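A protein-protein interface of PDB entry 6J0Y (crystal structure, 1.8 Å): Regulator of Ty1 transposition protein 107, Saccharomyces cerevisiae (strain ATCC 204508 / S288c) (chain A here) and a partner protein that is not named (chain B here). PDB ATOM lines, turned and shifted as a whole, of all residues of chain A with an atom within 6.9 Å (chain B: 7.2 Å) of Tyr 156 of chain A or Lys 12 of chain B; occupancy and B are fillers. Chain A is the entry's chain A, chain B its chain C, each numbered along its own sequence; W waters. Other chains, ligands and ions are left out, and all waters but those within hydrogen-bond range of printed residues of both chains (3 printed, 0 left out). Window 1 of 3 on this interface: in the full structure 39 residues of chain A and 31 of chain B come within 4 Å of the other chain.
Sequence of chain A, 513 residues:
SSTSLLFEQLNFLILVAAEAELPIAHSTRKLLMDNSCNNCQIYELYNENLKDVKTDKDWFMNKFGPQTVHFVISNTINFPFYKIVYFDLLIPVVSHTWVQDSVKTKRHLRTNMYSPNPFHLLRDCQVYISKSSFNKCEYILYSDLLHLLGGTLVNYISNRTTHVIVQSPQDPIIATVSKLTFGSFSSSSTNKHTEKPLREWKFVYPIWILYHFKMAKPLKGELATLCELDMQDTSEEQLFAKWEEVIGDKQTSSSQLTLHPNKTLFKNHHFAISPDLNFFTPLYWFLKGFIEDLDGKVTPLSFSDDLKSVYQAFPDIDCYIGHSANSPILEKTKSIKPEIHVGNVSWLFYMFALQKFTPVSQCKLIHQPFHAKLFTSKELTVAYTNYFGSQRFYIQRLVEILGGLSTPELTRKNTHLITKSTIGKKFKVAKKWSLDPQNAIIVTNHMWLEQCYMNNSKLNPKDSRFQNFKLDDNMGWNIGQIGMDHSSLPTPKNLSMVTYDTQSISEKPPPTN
The side-chain carboxylate (OE1) of Glu 40 of chain B is in salt-bridge range of the guanidinium group (NE) of Arg 160 of chain A, 3.1 Å away.
O of Ile 157 of chain A lies within hydrogen-bond range of N of Lys 12 of chain B (2.8 Å).
OE2 of Glu 40 of chain B is in hydrogen-bond range of NE2 of Gln 126 of chain A, 2.9 Å away.
The side-chain amide oxygen (OD1) of Asn 155 of chain A sits at hydrogen-bond distance from the guanidinium group (NH2) of Arg 10 of chain B (2.9 Å).
The backbone carbonyl oxygen (O) of Arg 10 of chain B lies within hydrogen-bond range of the backbone NH (N) of Ile 157 of chain A (2.8 Å).
OE1 of Glu 409 of chain A lies within salt-bridge range of NH1 of Arg 10 of chain B.
N of Ser 158 of chain A sits at hydrogen-bond distance from OG1 of Thr 161 of chain A (2.9 Å).
OG1 of Thr 407 of chain A sits at hydrogen-bond distance from O of Glu 409 of chain A, at 2.7 Å.
O of Ala 52 of chain B sits at hydrogen-bond distance from N of Val 11 of chain B.
OG of Ser 38 of chain B sits at hydrogen-bond distance from O of Glu 40 of chain B, at 2.8 Å.
The backbone carbonyl oxygen (O) of Leu 13 of chain B sits at hydrogen-bond distance from the backbone NH (N) of Cys 50 of chain B, 2.8 Å away.
N of Arg 160 of chain A sits close to OG of Ser 158 of chain A (3.1 Å).
Among the printed residues, merely in contact across the chains: Tyr 128 of chain A with Ile 9 of chain B (3.5 Å), Tyr 156 of chain A with Arg 10 of chain B (3.4 Å), Tyr 156 of chain A with Lys 12 of chain B (3.8 Å), Ile 157 of chain A with Val 11 of chain B (3.3 Å), Ser 158 of chain A with Lys 12 of chain B (3.9 Å), Leu 198 of chain A with Leu 13 of chain B (3.9 Å), Thr 407 of chain A with Arg 10 of chain B (3.6 Å), Pro 408 of chain A with Arg 10 of chain B (3.8 Å) and Glu 409 of chain A with Ile 51 of chain B (3.6 Å).
Of the printed residues of chain B, Gln 126 of chain A touches Glu 40.
Of chain B, only Arg 10 and Lys 12 come within 4 Å of Tyr 156 of chain A.
Printed residues of chain B within 4 Å of Glu 409 of chain A: Arg 10 (2.9 Å) and Ile 51 (3.6 Å).
Printed residues of chain A within 4 Å of Val 11 of chain B: Ile 157 (3.3 Å).
Of the printed residues of chain A, Lys 12 of chain B touches Tyr 156 (3.8 Å), Ile 157 (2.8 Å) and Ser 158 (3.9 Å).
Asp 37 of chain B touches none of the printed residues of chain A.
The nearest residue of chain A that does not touch Lys 12 of chain B is Asn 159 of chain A (4.8 Å).
Of the 17 printed residues of chain B, 7 touch a printed residue of chain A.
Hydrophobic or aromatic side chains of chain B that line the printed part of chain A: Ile 9, Val 11, Leu 13 and Ile 51.
Printed residues of chain A that touch a printed residue of chain B: Gln 126, Tyr 128, Asn 155, Tyr 156, Ile 157, Ser 158, Arg 160, Leu 198, Thr 407, Pro 408 and Glu 409.
Water W3 lies within hydrogen-bond range of the side-chain carboxylate (OE1) of Glu 40 of chain B (2.6 Å) and the side-chain amide oxygen (OE1) of Gln 126 of chain A (2.9 Å).
Water W1 bridges the backbone carbonyl oxygen (O) of Lys 12 of chain B and the backbone NH (N) of Asn 159 of chain A.
Water W2 lies within hydrogen-bond range of OH of Tyr 128 of chain A, O of Asn 155 of chain A and N of Arg 10 of chain B.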
ATOM      1  N   GLN A 126     -25.163  -7.815   3.480  1.00  0.00           N
ATOM      2  CA  GLN A 126     -25.586  -7.171   2.239  1.00  0.00           C
ATOM      3  C   GLN A 126     -25.400  -8.228   1.161  1.00  0.00           C
ATOM      4  O   GLN A 126     -24.273  -8.539   0.765  1.00  0.00           O
ATOM      5  CB  GLN A 126     -24.785  -5.902   1.957  1.00  0.00           C
ATOM      6  CG  GLN A 126     -24.959  -4.841   3.040  1.00  0.00           C
ATOM      7  CD  GLN A 126     -24.320  -3.519   2.688  1.00  0.00           C
ATOM      8  OE1 GLN A 126     -24.518  -2.993   1.593  1.00  0.00           O
ATOM      9  NE2 GLN A 126     -23.541  -2.969   3.623  1.00  0.00           N
ATOM     10  N   VAL A 127     -26.519  -8.797   0.724  1.00  0.00           N
ATOM     11  CA  VAL A 127     -26.532 -10.096   0.059  1.00  0.00           C
ATOM     12  C   VAL A 127     -27.019  -9.952  -1.369  1.00  0.00           C
ATOM     13  O   VAL A 127     -28.117  -9.435  -1.613  1.00  0.00           O
ATOM     14  CB  VAL A 127     -27.404 -11.091   0.834  1.00  0.00           C
ATOM     15  CG1 VAL A 127     -27.422 -12.442   0.124  1.00  0.00           C
ATOM     16  CG2 VAL A 127     -26.880 -11.229   2.277  1.00  0.00           C
ATOM     17  N   TYR A 128     -26.229 -10.485  -2.294  1.00  0.00           N
ATOM     18  CA  TYR A 128     -26.544 -10.531  -3.712  1.00  0.00           C
ATOM     19  C   TYR A 128     -26.979 -11.953  -4.054  1.00  0.00           C
ATOM     20  O   TYR A 128     -26.216 -12.895  -3.839  1.00  0.00           O
ATOM     21  CB  TYR A 128     -25.309 -10.143  -4.522  1.00  0.00           C
ATOM     22  CG  TYR A 128     -25.555 -10.064  -6.026  1.00  0.00           C
ATOM     23  CD1 TYR A 128     -25.606 -11.221  -6.801  1.00  0.00           C
ATOM     24  CD2 TYR A 128     -25.743  -8.843  -6.647  1.00  0.00           C
ATOM     25  CE1 TYR A 128     -25.843 -11.165  -8.166  1.00  0.00           C
ATOM     26  CE2 TYR A 128     -25.978  -8.766  -8.041  1.00  0.00           C
ATOM     27  CZ  TYR A 128     -26.027  -9.936  -8.779  1.00  0.00           C
ATOM     28  OH  TYR A 128     -26.252  -9.870 -10.137  1.00  0.00           O
ATOM     29  N   THR A 152     -30.044  -7.155   4.055  1.00  0.00           N
ATOM     30  CA  THR A 152     -30.303  -6.260   2.938  1.00  0.00           C
ATOM     31  C   THR A 152     -30.064  -7.003   1.630  1.00  0.00           C
ATOM     32  O   THR A 152     -29.001  -7.598   1.436  1.00  0.00           O
ATOM     33  CB  THR A 152     -29.398  -5.031   3.014  1.00  0.00           C
ATOM     34  OG1 THR A 152     -29.664  -4.327   4.231  1.00  0.00           O
ATOM     35  CG2 THR A 152     -29.659  -4.110   1.834  1.00  0.00           C
ATOM     36  N   LEU A 153     -31.037  -6.940   0.734  1.00  0.00           N
ATOM     37  CA  LEU A 153     -30.892  -7.472  -0.613  1.00  0.00           C
ATOM     38  C   LEU A 153     -30.291  -6.403  -1.527  1.00  0.00           C
ATOM     39  O   LEU A 153     -30.774  -5.270  -1.549  1.00  0.00           O
ATOM     40  CB  LEU A 153     -32.258  -7.899  -1.142  1.00  0.00           C
ATOM     41  CG  LEU A 153     -32.280  -8.413  -2.581  1.00  0.00           C
ATOM     42  CD1 LEU A 153     -31.559  -9.745  -2.671  1.00  0.00           C
ATOM     43  CD2 LEU A 153     -33.718  -8.538  -3.101  1.00  0.00           C
ATOM     44  N   VAL A 154     -29.251  -6.762  -2.285  1.00  0.00           N
ATOM     45  CA  VAL A 154     -28.677  -5.867  -3.289  1.00  0.00           C
ATOM     46  C   VAL A 154     -28.730  -6.544  -4.648  1.00  0.00           C
ATOM     47  O   VAL A 154     -28.560  -7.765  -4.750  1.00  0.00           O
ATOM     48  CB  VAL A 154     -27.231  -5.439  -2.965  1.00  0.00           C
ATOM     49  CG1 VAL A 154     -27.236  -4.502  -1.749  1.00  0.00           C
ATOM     50  CG2 VAL A 154     -26.305  -6.649  -2.725  1.00  0.00           C
ATOM     51  N   ASN A 155     -28.973  -5.744  -5.697  1.00  0.00           N
ATOM     52  CA  ASN A 155     -28.968  -6.261  -7.064  1.00  0.00           C
ATOM     53  C   ASN A 155     -27.743  -5.790  -7.838  1.00  0.00           C
ATOM     54  O   ASN A 155     -27.737  -5.800  -9.081  1.00  0.00           O
ATOM     55  CB  ASN A 155     -30.266  -5.900  -7.807  1.00  0.00           C
ATOM     56  CG  ASN A 155     -30.492  -4.392  -7.936  1.00  0.00           C
ATOM     57  OD1 ASN A 155     -29.573  -3.600  -7.783  1.00  0.00           O
ATOM     58  ND2 ASN A 155     -31.729  -4.003  -8.236  1.00  0.00           N
ATOM     59  N   TYR A 156     -26.708  -5.363  -7.117  1.00  0.00           N
ATOM     60  CA  TYR A 156     -25.445  -4.936  -7.692  1.00  0.00           C
ATOM     61  C   TYR A 156     -24.329  -5.448  -6.791  1.00  0.00           C
ATOM     62  O   TYR A 156     -24.478  -5.507  -5.558  1.00  0.00           O
ATOM     63  CB  TYR A 156     -25.367  -3.386  -7.818  1.00  0.00           C
ATOM     64  CG  TYR A 156     -25.486  -2.704  -6.465  1.00  0.00           C
ATOM     65  CD1 TYR A 156     -26.728  -2.544  -5.845  1.00  0.00           C
ATOM     66  CD2 TYR A 156     -24.351  -2.257  -5.788  1.00  0.00           C
ATOM     67  CE1 TYR A 156     -26.839  -1.954  -4.582  1.00  0.00           C
ATOM     68  CE2 TYR A 156     -24.451  -1.648  -4.502  1.00  0.00           C
ATOM     69  CZ  TYR A 156     -25.696  -1.509  -3.919  1.00  0.00           C
ATOM     70  OH  TYR A 156     -25.808  -0.922  -2.671  1.00  0.00           O
ATOM     71  N   ILE A 157     -23.203  -5.794  -7.421  1.00  0.00           N
ATOM     72  CA  ILE A 157     -21.970  -6.192  -6.745  1.00  0.00           C
ATOM     73  C   ILE A 157     -21.163  -4.941  -6.405  1.00  0.00           C
ATOM     74  O   ILE A 157     -21.052  -4.014  -7.213  1.00  0.00           O
ATOM     75  CB  ILE A 157     -21.154  -7.149  -7.637  1.00  0.00           C
ATOM     76  CG1 ILE A 157     -21.896  -8.479  -7.865  1.00  0.00           C
ATOM     77  CG2 ILE A 157     -19.747  -7.359  -7.068  1.00  0.00           C
ATOM     78  CD1 ILE A 157     -22.059  -9.345  -6.578  1.00  0.00           C
ATOM     79  N   SER A 158     -20.580  -4.900  -5.208  1.00  0.00           N
ATOM     80  CA  SER A 158     -19.732  -3.774  -4.836  1.00  0.00           C
ATOM     81  C   SER A 158     -18.720  -4.258  -3.810  1.00  0.00           C
ATOM     82  O   SER A 158     -18.747  -5.416  -3.386  1.00  0.00           O
ATOM     83  CB  SER A 158     -20.559  -2.608  -4.284  1.00  0.00           C
ATOM     84  OG  SER A 158     -21.083  -2.923  -3.001  1.00  0.00           O
ATOM     85  N   ASN A 159     -17.835  -3.357  -3.387  1.00  0.00           N
ATOM     86  CA  ASN A 159     -16.953  -3.778  -2.298  1.00  0.00           C
ATOM     87  C   ASN A 159     -17.670  -3.875  -0.950  1.00  0.00           C
ATOM     88  O   ASN A 159     -17.012  -4.183   0.052  1.00  0.00           O
ATOM     89  CB  ASN A 159     -15.744  -2.847  -2.187  1.00  0.00           C
ATOM     90  CG  ASN A 159     -16.115  -1.449  -1.755  1.00  0.00           C
ATOM     91  OD1 ASN A 159     -17.286  -1.133  -1.542  1.00  0.00           O
ATOM     92  ND2 ASN A 159     -15.108  -0.597  -1.613  1.00  0.00           N
ATOM     93  N   ARG A 160     -18.983  -3.641  -0.891  1.00  0.00           N
ATOM     94  CA  ARG A 160     -19.750  -3.844   0.335  1.00  0.00           C
ATOM     95  C   ARG A 160     -20.615  -5.101   0.308  1.00  0.00           C
ATOM     96  O   ARG A 160     -21.329  -5.358   1.282  1.00  0.00           O
ATOM     97  CB  ARG A 160     -20.641  -2.627   0.622  1.00  0.00           C
ATOM     98  CG  ARG A 160     -19.899  -1.276   0.599  1.00  0.00           C
ATOM     99  CD  ARG A 160     -18.818  -1.244   1.660  1.00  0.00           C
ATOM    100  NE  ARG A 160     -19.414  -1.254   2.992  1.00  0.00           N
ATOM    101  CZ  ARG A 160     -18.787  -1.645   4.098  1.00  0.00           C
ATOM    102  NH1 ARG A 160     -17.530  -2.070   4.042  1.00  0.00           N
ATOM    103  NH2 ARG A 160     -19.424  -1.617   5.260  1.00  0.00           N
ATOM    104  N   THR A 161     -20.593  -5.877  -0.778  1.00  0.00           N
ATOM    105  CA  THR A 161     -21.354  -7.125  -0.828  1.00  0.00           C
ATOM    106  C   THR A 161     -20.745  -8.144   0.130  1.00  0.00           C
ATOM    107  O   THR A 161     -19.619  -8.599  -0.093  1.00  0.00           O
ATOM    108  CB  THR A 161     -21.346  -7.711  -2.238  1.00  0.00           C
ATOM    109  OG1 THR A 161     -21.709  -6.714  -3.203  1.00  0.00           O
ATOM    110  CG2 THR A 161     -22.331  -8.886  -2.322  1.00  0.00           C
ATOM    111  N   LEU A 198     -11.595  -6.413  -5.982  1.00  0.00           N
ATOM    112  CA  LEU A 198     -12.560  -5.454  -5.453  1.00  0.00           C
ATOM    113  C   LEU A 198     -12.798  -5.687  -3.966  1.00  0.00           C
ATOM    114  O   LEU A 198     -12.912  -4.732  -3.190  1.00  0.00           O
ATOM    115  CB  LEU A 198     -13.871  -5.542  -6.238  1.00  0.00           C
ATOM    116  CG  LEU A 198     -15.005  -4.581  -5.877  1.00  0.00           C
ATOM    117  CD1 LEU A 198     -14.585  -3.116  -6.046  1.00  0.00           C
ATOM    118  CD2 LEU A 198     -16.226  -4.884  -6.728  1.00  0.00           C
ATOM    119  N   THR A 407     -33.285   0.314  -8.834  1.00  0.00           N
ATOM    120  CA  THR A 407     -31.890   0.655  -8.566  1.00  0.00           C
ATOM    121  C   THR A 407     -31.878   1.572  -7.340  1.00  0.00           C
ATOM    122  O   THR A 407     -32.708   2.489  -7.246  1.00  0.00           O
ATOM    123  CB  THR A 407     -31.188   1.332  -9.770  1.00  0.00           C
ATOM    124  OG1 THR A 407     -31.770   2.615 -10.043  1.00  0.00           O
ATOM    125  CG2 THR A 407     -31.256   0.444 -11.055  1.00  0.00           C
ATOM    126  N   PRO A 408     -30.990   1.333  -6.368  1.00  0.00           N
ATOM    127  CA  PRO A 408     -30.825   2.313  -5.276  1.00  0.00           C
ATOM    128  C   PRO A 408     -30.067   3.540  -5.708  1.00  0.00           C
ATOM    129  O   PRO A 408     -30.191   4.590  -5.064  1.00  0.00           O
ATOM    130  CB  PRO A 408     -30.038   1.541  -4.197  1.00  0.00           C
ATOM    131  CG  PRO A 408     -29.953   0.104  -4.689  1.00  0.00           C
ATOM    132  CD  PRO A 408     -30.216   0.095  -6.166  1.00  0.00           C
ATOM    133  N   GLU A 409     -29.281   3.437  -6.771  1.00  0.00           N
ATOM    134  CA  GLU A 409     -28.538   4.559  -7.306  1.00  0.00           C
ATOM    135  C   GLU A 409     -29.326   5.211  -8.440  1.00  0.00           C
ATOM    136  O   GLU A 409     -30.198   4.594  -9.061  1.00  0.00           O
ATOM    137  CB  GLU A 409     -27.160   4.094  -7.795  1.00  0.00           C
ATOM    138  CG  GLU A 409     -27.110   3.544  -9.250  1.00  0.00           C
ATOM    139  CD  GLU A 409     -27.733   2.155  -9.434  1.00  0.00           C
ATOM    140  OE1 GLU A 409     -28.054   1.789 -10.601  1.00  0.00           O
ATOM    141  OE2 GLU A 409     -27.888   1.416  -8.445  1.00  0.00           O
ATOM    142  N   ILE B   9     -24.214  -8.500 -15.167  1.00  0.00           N
ATOM    143  CA  ILE B   9     -24.471  -8.160 -13.774  1.00  0.00           C
ATOM    144  C   ILE B   9     -24.072  -6.709 -13.579  1.00  0.00           C
ATOM    145  O   ILE B   9     -23.217  -6.177 -14.297  1.00  0.00           O
ATOM    146  CB  ILE B   9     -23.697  -9.066 -12.794  1.00  0.00           C
ATOM    147  CG1 ILE B   9     -22.187  -8.936 -13.036  1.00  0.00           C
ATOM    148  CG2 ILE B   9     -24.156 -10.531 -12.924  1.00  0.00           C
ATOM    149  CD1 ILE B   9     -21.349  -9.729 -12.031  1.00  0.00           C
ATOM    150  N   ARG B  10     -24.676  -6.082 -12.574  1.00  0.00           N
ATOM    151  CA  ARG B  10     -24.390  -4.698 -12.198  1.00  0.00           C
ATOM    152  C   ARG B  10     -23.244  -4.662 -11.196  1.00  0.00           C
ATOM    153  O   ARG B  10     -23.273  -5.393 -10.207  1.00  0.00           O
ATOM    154  CB  ARG B  10     -25.632  -4.061 -11.566  1.00  0.00           C
ATOM    155  CG  ARG B  10     -26.730  -3.704 -12.581  1.00  0.00           C
ATOM    156  CD  ARG B  10     -28.124  -3.772 -11.950  1.00  0.00           C
ATOM    157  NE  ARG B  10     -28.260  -3.120 -10.640  1.00  0.00           N
ATOM    158  CZ  ARG B  10     -28.186  -1.810 -10.415  1.00  0.00           C
ATOM    159  NH1 ARG B  10     -27.919  -0.958 -11.408  1.00  0.00           N
ATOM    160  NH2 ARG B  10     -28.366  -1.367  -9.169  1.00  0.00           N
ATOM    161  N   VAL B  11     -22.246  -3.810 -11.448  1.00  0.00           N
ATOM    162  CA  VAL B  11     -21.116  -3.632 -10.538  1.00  0.00           C
ATOM    163  C   VAL B  11     -20.954  -2.146 -10.256  1.00  0.00           C
ATOM    164  O   VAL B  11     -20.806  -1.350 -11.189  1.00  0.00           O
ATOM    165  CB  VAL B  11     -19.805  -4.210 -11.098  1.00  0.00           C
ATOM    166  CG1 VAL B  11     -18.703  -4.109 -10.040  1.00  0.00           C
ATOM    167  CG2 VAL B  11     -19.985  -5.680 -11.517  1.00  0.00           C
ATOM    168  N   LYS B  12     -20.982  -1.779  -8.973  1.00  0.00           N
ATOM    169  CA  LYS B  12     -20.788  -0.392  -8.548  1.00  0.00           C
ATOM    170  C   LYS B  12     -19.320  -0.190  -8.209  1.00  0.00           C
ATOM    171  O   LYS B  12     -18.795  -0.848  -7.306  1.00  0.00           O
ATOM    172  CB  LYS B  12     -21.663  -0.064  -7.342  1.00  0.00           C
ATOM    173  CG  LYS B  12     -21.522   1.403  -6.850  1.00  0.00           C
ATOM    174  CD  LYS B  12     -22.303   1.568  -5.567  1.00  0.00           C
ATOM    175  CE  LYS B  12     -22.051   2.943  -4.929  1.00  0.00           C
ATOM    176  NZ  LYS B  12     -22.766   3.002  -3.629  1.00  0.00           N
ATOM    177  N   LEU B  13     -18.680   0.743  -8.915  1.00  0.00           N
ATOM    178  CA  LEU B  13     -17.240   0.951  -8.909  1.00  0.00           C
ATOM    179  C   LEU B  13     -16.951   2.438  -8.760  1.00  0.00           C
ATOM    180  O   LEU B  13     -17.686   3.268  -9.288  1.00  0.00           O
ATOM    181  CB  LEU B  13     -16.627   0.483 -10.245  1.00  0.00           C
ATOM    182  CG  LEU B  13     -15.674  -0.693 -10.318  1.00  0.00           C
ATOM    183  CD1 LEU B  13     -16.135  -1.781  -9.380  1.00  0.00           C
ATOM    184  CD2 LEU B  13     -15.610  -1.195 -11.755  1.00  0.00           C
ATOM    185  N   LEU B  14     -15.853   2.776  -8.088  1.00  0.00           N
ATOM    186  CA  LEU B  14     -15.362   4.151  -8.163  1.00  0.00           C
ATOM    187  C   LEU B  14     -15.035   4.503  -9.611  1.00  0.00           C
ATOM    188  O   LEU B  14     -14.451   3.700 -10.343  1.00  0.00           O
ATOM    189  CB  LEU B  14     -14.122   4.331  -7.281  1.00  0.00           C
ATOM    190  CG  LEU B  14     -14.388   4.477  -5.783  1.00  0.00           C
ATOM    191  CD1 LEU B  14     -13.081   4.545  -4.991  1.00  0.00           C
ATOM    192  CD2 LEU B  14     -15.232   5.719  -5.520  1.00  0.00           C
ATOM    193  N   VAL B  33     -22.871   7.670 -11.877  1.00  0.00           N
ATOM    194  CA  VAL B  33     -23.846   7.785 -10.799  1.00  0.00           C
ATOM    195  C   VAL B  33     -23.935   9.251 -10.385  1.00  0.00           C
ATOM    196  O   VAL B  33     -22.916   9.941 -10.293  1.00  0.00           O
ATOM    197  CB  VAL B  33     -23.454   6.876  -9.613  1.00  0.00           C
ATOM    198  CG1 VAL B  33     -24.315   7.191  -8.354  1.00  0.00           C
ATOM    199  CG2 VAL B  33     -23.579   5.390  -9.993  1.00  0.00           C
ATOM    200  N   ASN B  36     -25.322  10.570  -5.363  1.00  0.00           N
ATOM    201  CA  ASN B  36     -25.029   9.480  -4.446  1.00  0.00           C
ATOM    202  C   ASN B  36     -25.167   9.933  -2.994  1.00  0.00           C
ATOM    203  O   ASN B  36     -24.737  11.028  -2.623  1.00  0.00           O
ATOM    204  CB  ASN B  36     -23.615   8.966  -4.689  1.00  0.00           C
ATOM    205  CG  ASN B  36     -23.240   7.854  -3.740  1.00  0.00           C
ATOM    206  OD1 ASN B  36     -23.728   6.739  -3.874  1.00  0.00           O
ATOM    207  ND2 ASN B  36     -22.375   8.154  -2.776  1.00  0.00           N
ATOM    208  N   ASP B  37     -25.784   9.082  -2.175  1.00  0.00           N
ATOM    209  CA  ASP B  37     -25.920   9.316  -0.736  1.00  0.00           C
ATOM    210  C   ASP B  37     -25.101   8.268   0.002  1.00  0.00           C
ATOM    211  O   ASP B  37     -25.402   7.075  -0.079  1.00  0.00           O
ATOM    212  CB  ASP B  37     -27.382   9.224  -0.293  1.00  0.00           C
ATOM    213  CG  ASP B  37     -28.232  10.352  -0.831  1.00  0.00           C
ATOM    214  OD1 ASP B  37     -27.885  11.523  -0.577  1.00  0.00           O
ATOM    215  OD2 ASP B  37     -29.241  10.056  -1.512  1.00  0.00           O
ATOM    216  N   SER B  38     -24.075   8.700   0.717  1.00  0.00           N
ATOM    217  CA  SER B  38     -23.321   7.754   1.527  1.00  0.00           C
ATOM    218  C   SER B  38     -24.148   7.374   2.746  1.00  0.00           C
ATOM    219  O   SER B  38     -24.568   8.245   3.517  1.00  0.00           O
ATOM    220  CB  SER B  38     -21.986   8.349   1.961  1.00  0.00           C
ATOM    221  OG  SER B  38     -21.452   7.595   3.041  1.00  0.00           O
ATOM    222  N   GLU B  39     -24.398   6.076   2.925  1.00  0.00           N
ATOM    223  CA  GLU B  39     -25.074   5.622   4.133  1.00  0.00           C
ATOM    224  C   GLU B  39     -24.158   4.796   5.029  1.00  0.00           C
ATOM    225  O   GLU B  39     -24.640   4.126   5.949  1.00  0.00           O
ATOM    226  CB  GLU B  39     -26.346   4.846   3.782  1.00  0.00           C
ATOM    227  CG  GLU B  39     -26.179   3.817   2.690  1.00  0.00           C
ATOM    228  CD  GLU B  39     -27.467   3.052   2.401  1.00  0.00           C
ATOM    229  OE1 GLU B  39     -27.384   1.970   1.783  1.00  0.00           O
ATOM    230  OE2 GLU B  39     -28.558   3.527   2.791  1.00  0.00           O
ATOM    231  N   GLU B  40     -22.847   4.824   4.773  1.00  0.00           N
ATOM    232  CA  GLU B  40     -21.868   4.153   5.625  1.00  0.00           C
ATOM    233  C   GLU B  40     -20.614   5.016   5.739  1.00  0.00           C
ATOM    234  O   GLU B  40     -20.239   5.727   4.798  1.00  0.00           O
ATOM    235  CB  GLU B  40     -21.486   2.762   5.078  1.00  0.00           C
ATOM    236  CG  GLU B  40     -22.669   1.830   4.810  1.00  0.00           C
ATOM    237  CD  GLU B  40     -22.274   0.574   4.055  1.00  0.00           C
ATOM    238  OE1 GLU B  40     -21.876   0.686   2.876  1.00  0.00           O
ATOM    239  OE2 GLU B  40     -22.356  -0.526   4.644  1.00  0.00           O
ATOM    240  N   THR B  43     -17.946   4.856   2.951  1.00  0.00           N
ATOM    241  CA  THR B  43     -18.090   5.653   1.739  1.00  0.00           C
ATOM    242  C   THR B  43     -17.957   7.127   2.091  1.00  0.00           C
ATOM    243  O   THR B  43     -18.602   7.605   3.030  1.00  0.00           O
ATOM    244  CB  THR B  43     -19.439   5.398   1.062  1.00  0.00           C
ATOM    245  OG1 THR B  43     -19.580   4.000   0.792  1.00  0.00           O
ATOM    246  CG2 THR B  43     -19.542   6.175  -0.262  1.00  0.00           C
ATOM    247  N   PHE B  49     -19.069   7.507  -8.194  1.00  0.00           N
ATOM    248  CA  PHE B  49     -19.236   6.129  -8.609  1.00  0.00           C
ATOM    249  C   PHE B  49     -19.769   6.033 -10.032  1.00  0.00           C
ATOM    250  O   PHE B  49     -20.286   6.987 -10.620  1.00  0.00           O
ATOM    251  CB  PHE B  49     -20.191   5.388  -7.671  1.00  0.00           C
ATOM    252  CG  PHE B  49     -19.633   5.169  -6.292  1.00  0.00           C
ATOM    253  CD1 PHE B  49     -18.764   4.119  -6.049  1.00  0.00           C
ATOM    254  CD2 PHE B  49     -19.972   6.007  -5.255  1.00  0.00           C
ATOM    255  CE1 PHE B  49     -18.241   3.907  -4.771  1.00  0.00           C
ATOM    256  CE2 PHE B  49     -19.450   5.811  -3.982  1.00  0.00           C
ATOM    257  CZ  PHE B  49     -18.583   4.765  -3.745  1.00  0.00           C
ATOM    258  N   CYS B  50     -19.642   4.829 -10.563  1.00  0.00           N
ATOM    259  CA  CYS B  50     -20.316   4.450 -11.790  1.00  0.00           C
ATOM    260  C   CYS B  50     -20.899   3.060 -11.595  1.00  0.00           C
ATOM    261  O   CYS B  50     -20.512   2.326 -10.686  1.00  0.00           O
ATOM    262  CB  CYS B  50     -19.367   4.440 -12.977  1.00  0.00           C
ATOM    263  SG  CYS B  50     -18.141   3.192 -12.740  1.00  0.00           S
ATOM    264  N   ILE B  51     -21.860   2.725 -12.448  1.00  0.00           N
ATOM    265  CA  ILE B  51     -22.404   1.378 -12.537  1.00  0.00           C
ATOM    266  C   ILE B  51     -21.925   0.806 -13.862  1.00  0.00           C
ATOM    267  O   ILE B  51     -22.088   1.443 -14.909  1.00  0.00           O
ATOM    268  CB  ILE B  51     -23.942   1.356 -12.468  1.00  0.00           C
ATOM    269  CG1 ILE B  51     -24.443   1.839 -11.105  1.00  0.00           C
ATOM    270  CG2 ILE B  51     -24.468  -0.069 -12.775  1.00  0.00           C
ATOM    271  CD1 ILE B  51     -24.048   0.929  -9.930  1.00  0.00           C
ATOM    272  N   ALA B  52     -21.312  -0.369 -13.817  1.00  0.00           N
ATOM    273  CA  ALA B  52     -20.936  -1.095 -15.022  1.00  0.00           C
ATOM    274  C   ALA B  52     -21.802  -2.341 -15.162  1.00  0.00           C
ATOM    275  O   ALA B  52     -22.015  -3.071 -14.187  1.00  0.00           O
ATOM    276  CB  ALA B  52     -19.456  -1.482 -14.985  1.00  0.00           C
HETATM  277  O   HOH W   1     -17.547  -0.871  -4.901  1.00  0.00           O
HETATM  278  O   HOH W   2     -26.902  -7.420 -11.146  1.00  0.00           O
HETATM  279  O   HOH W   3     -23.452  -0.321   1.081  1.00  0.00           O
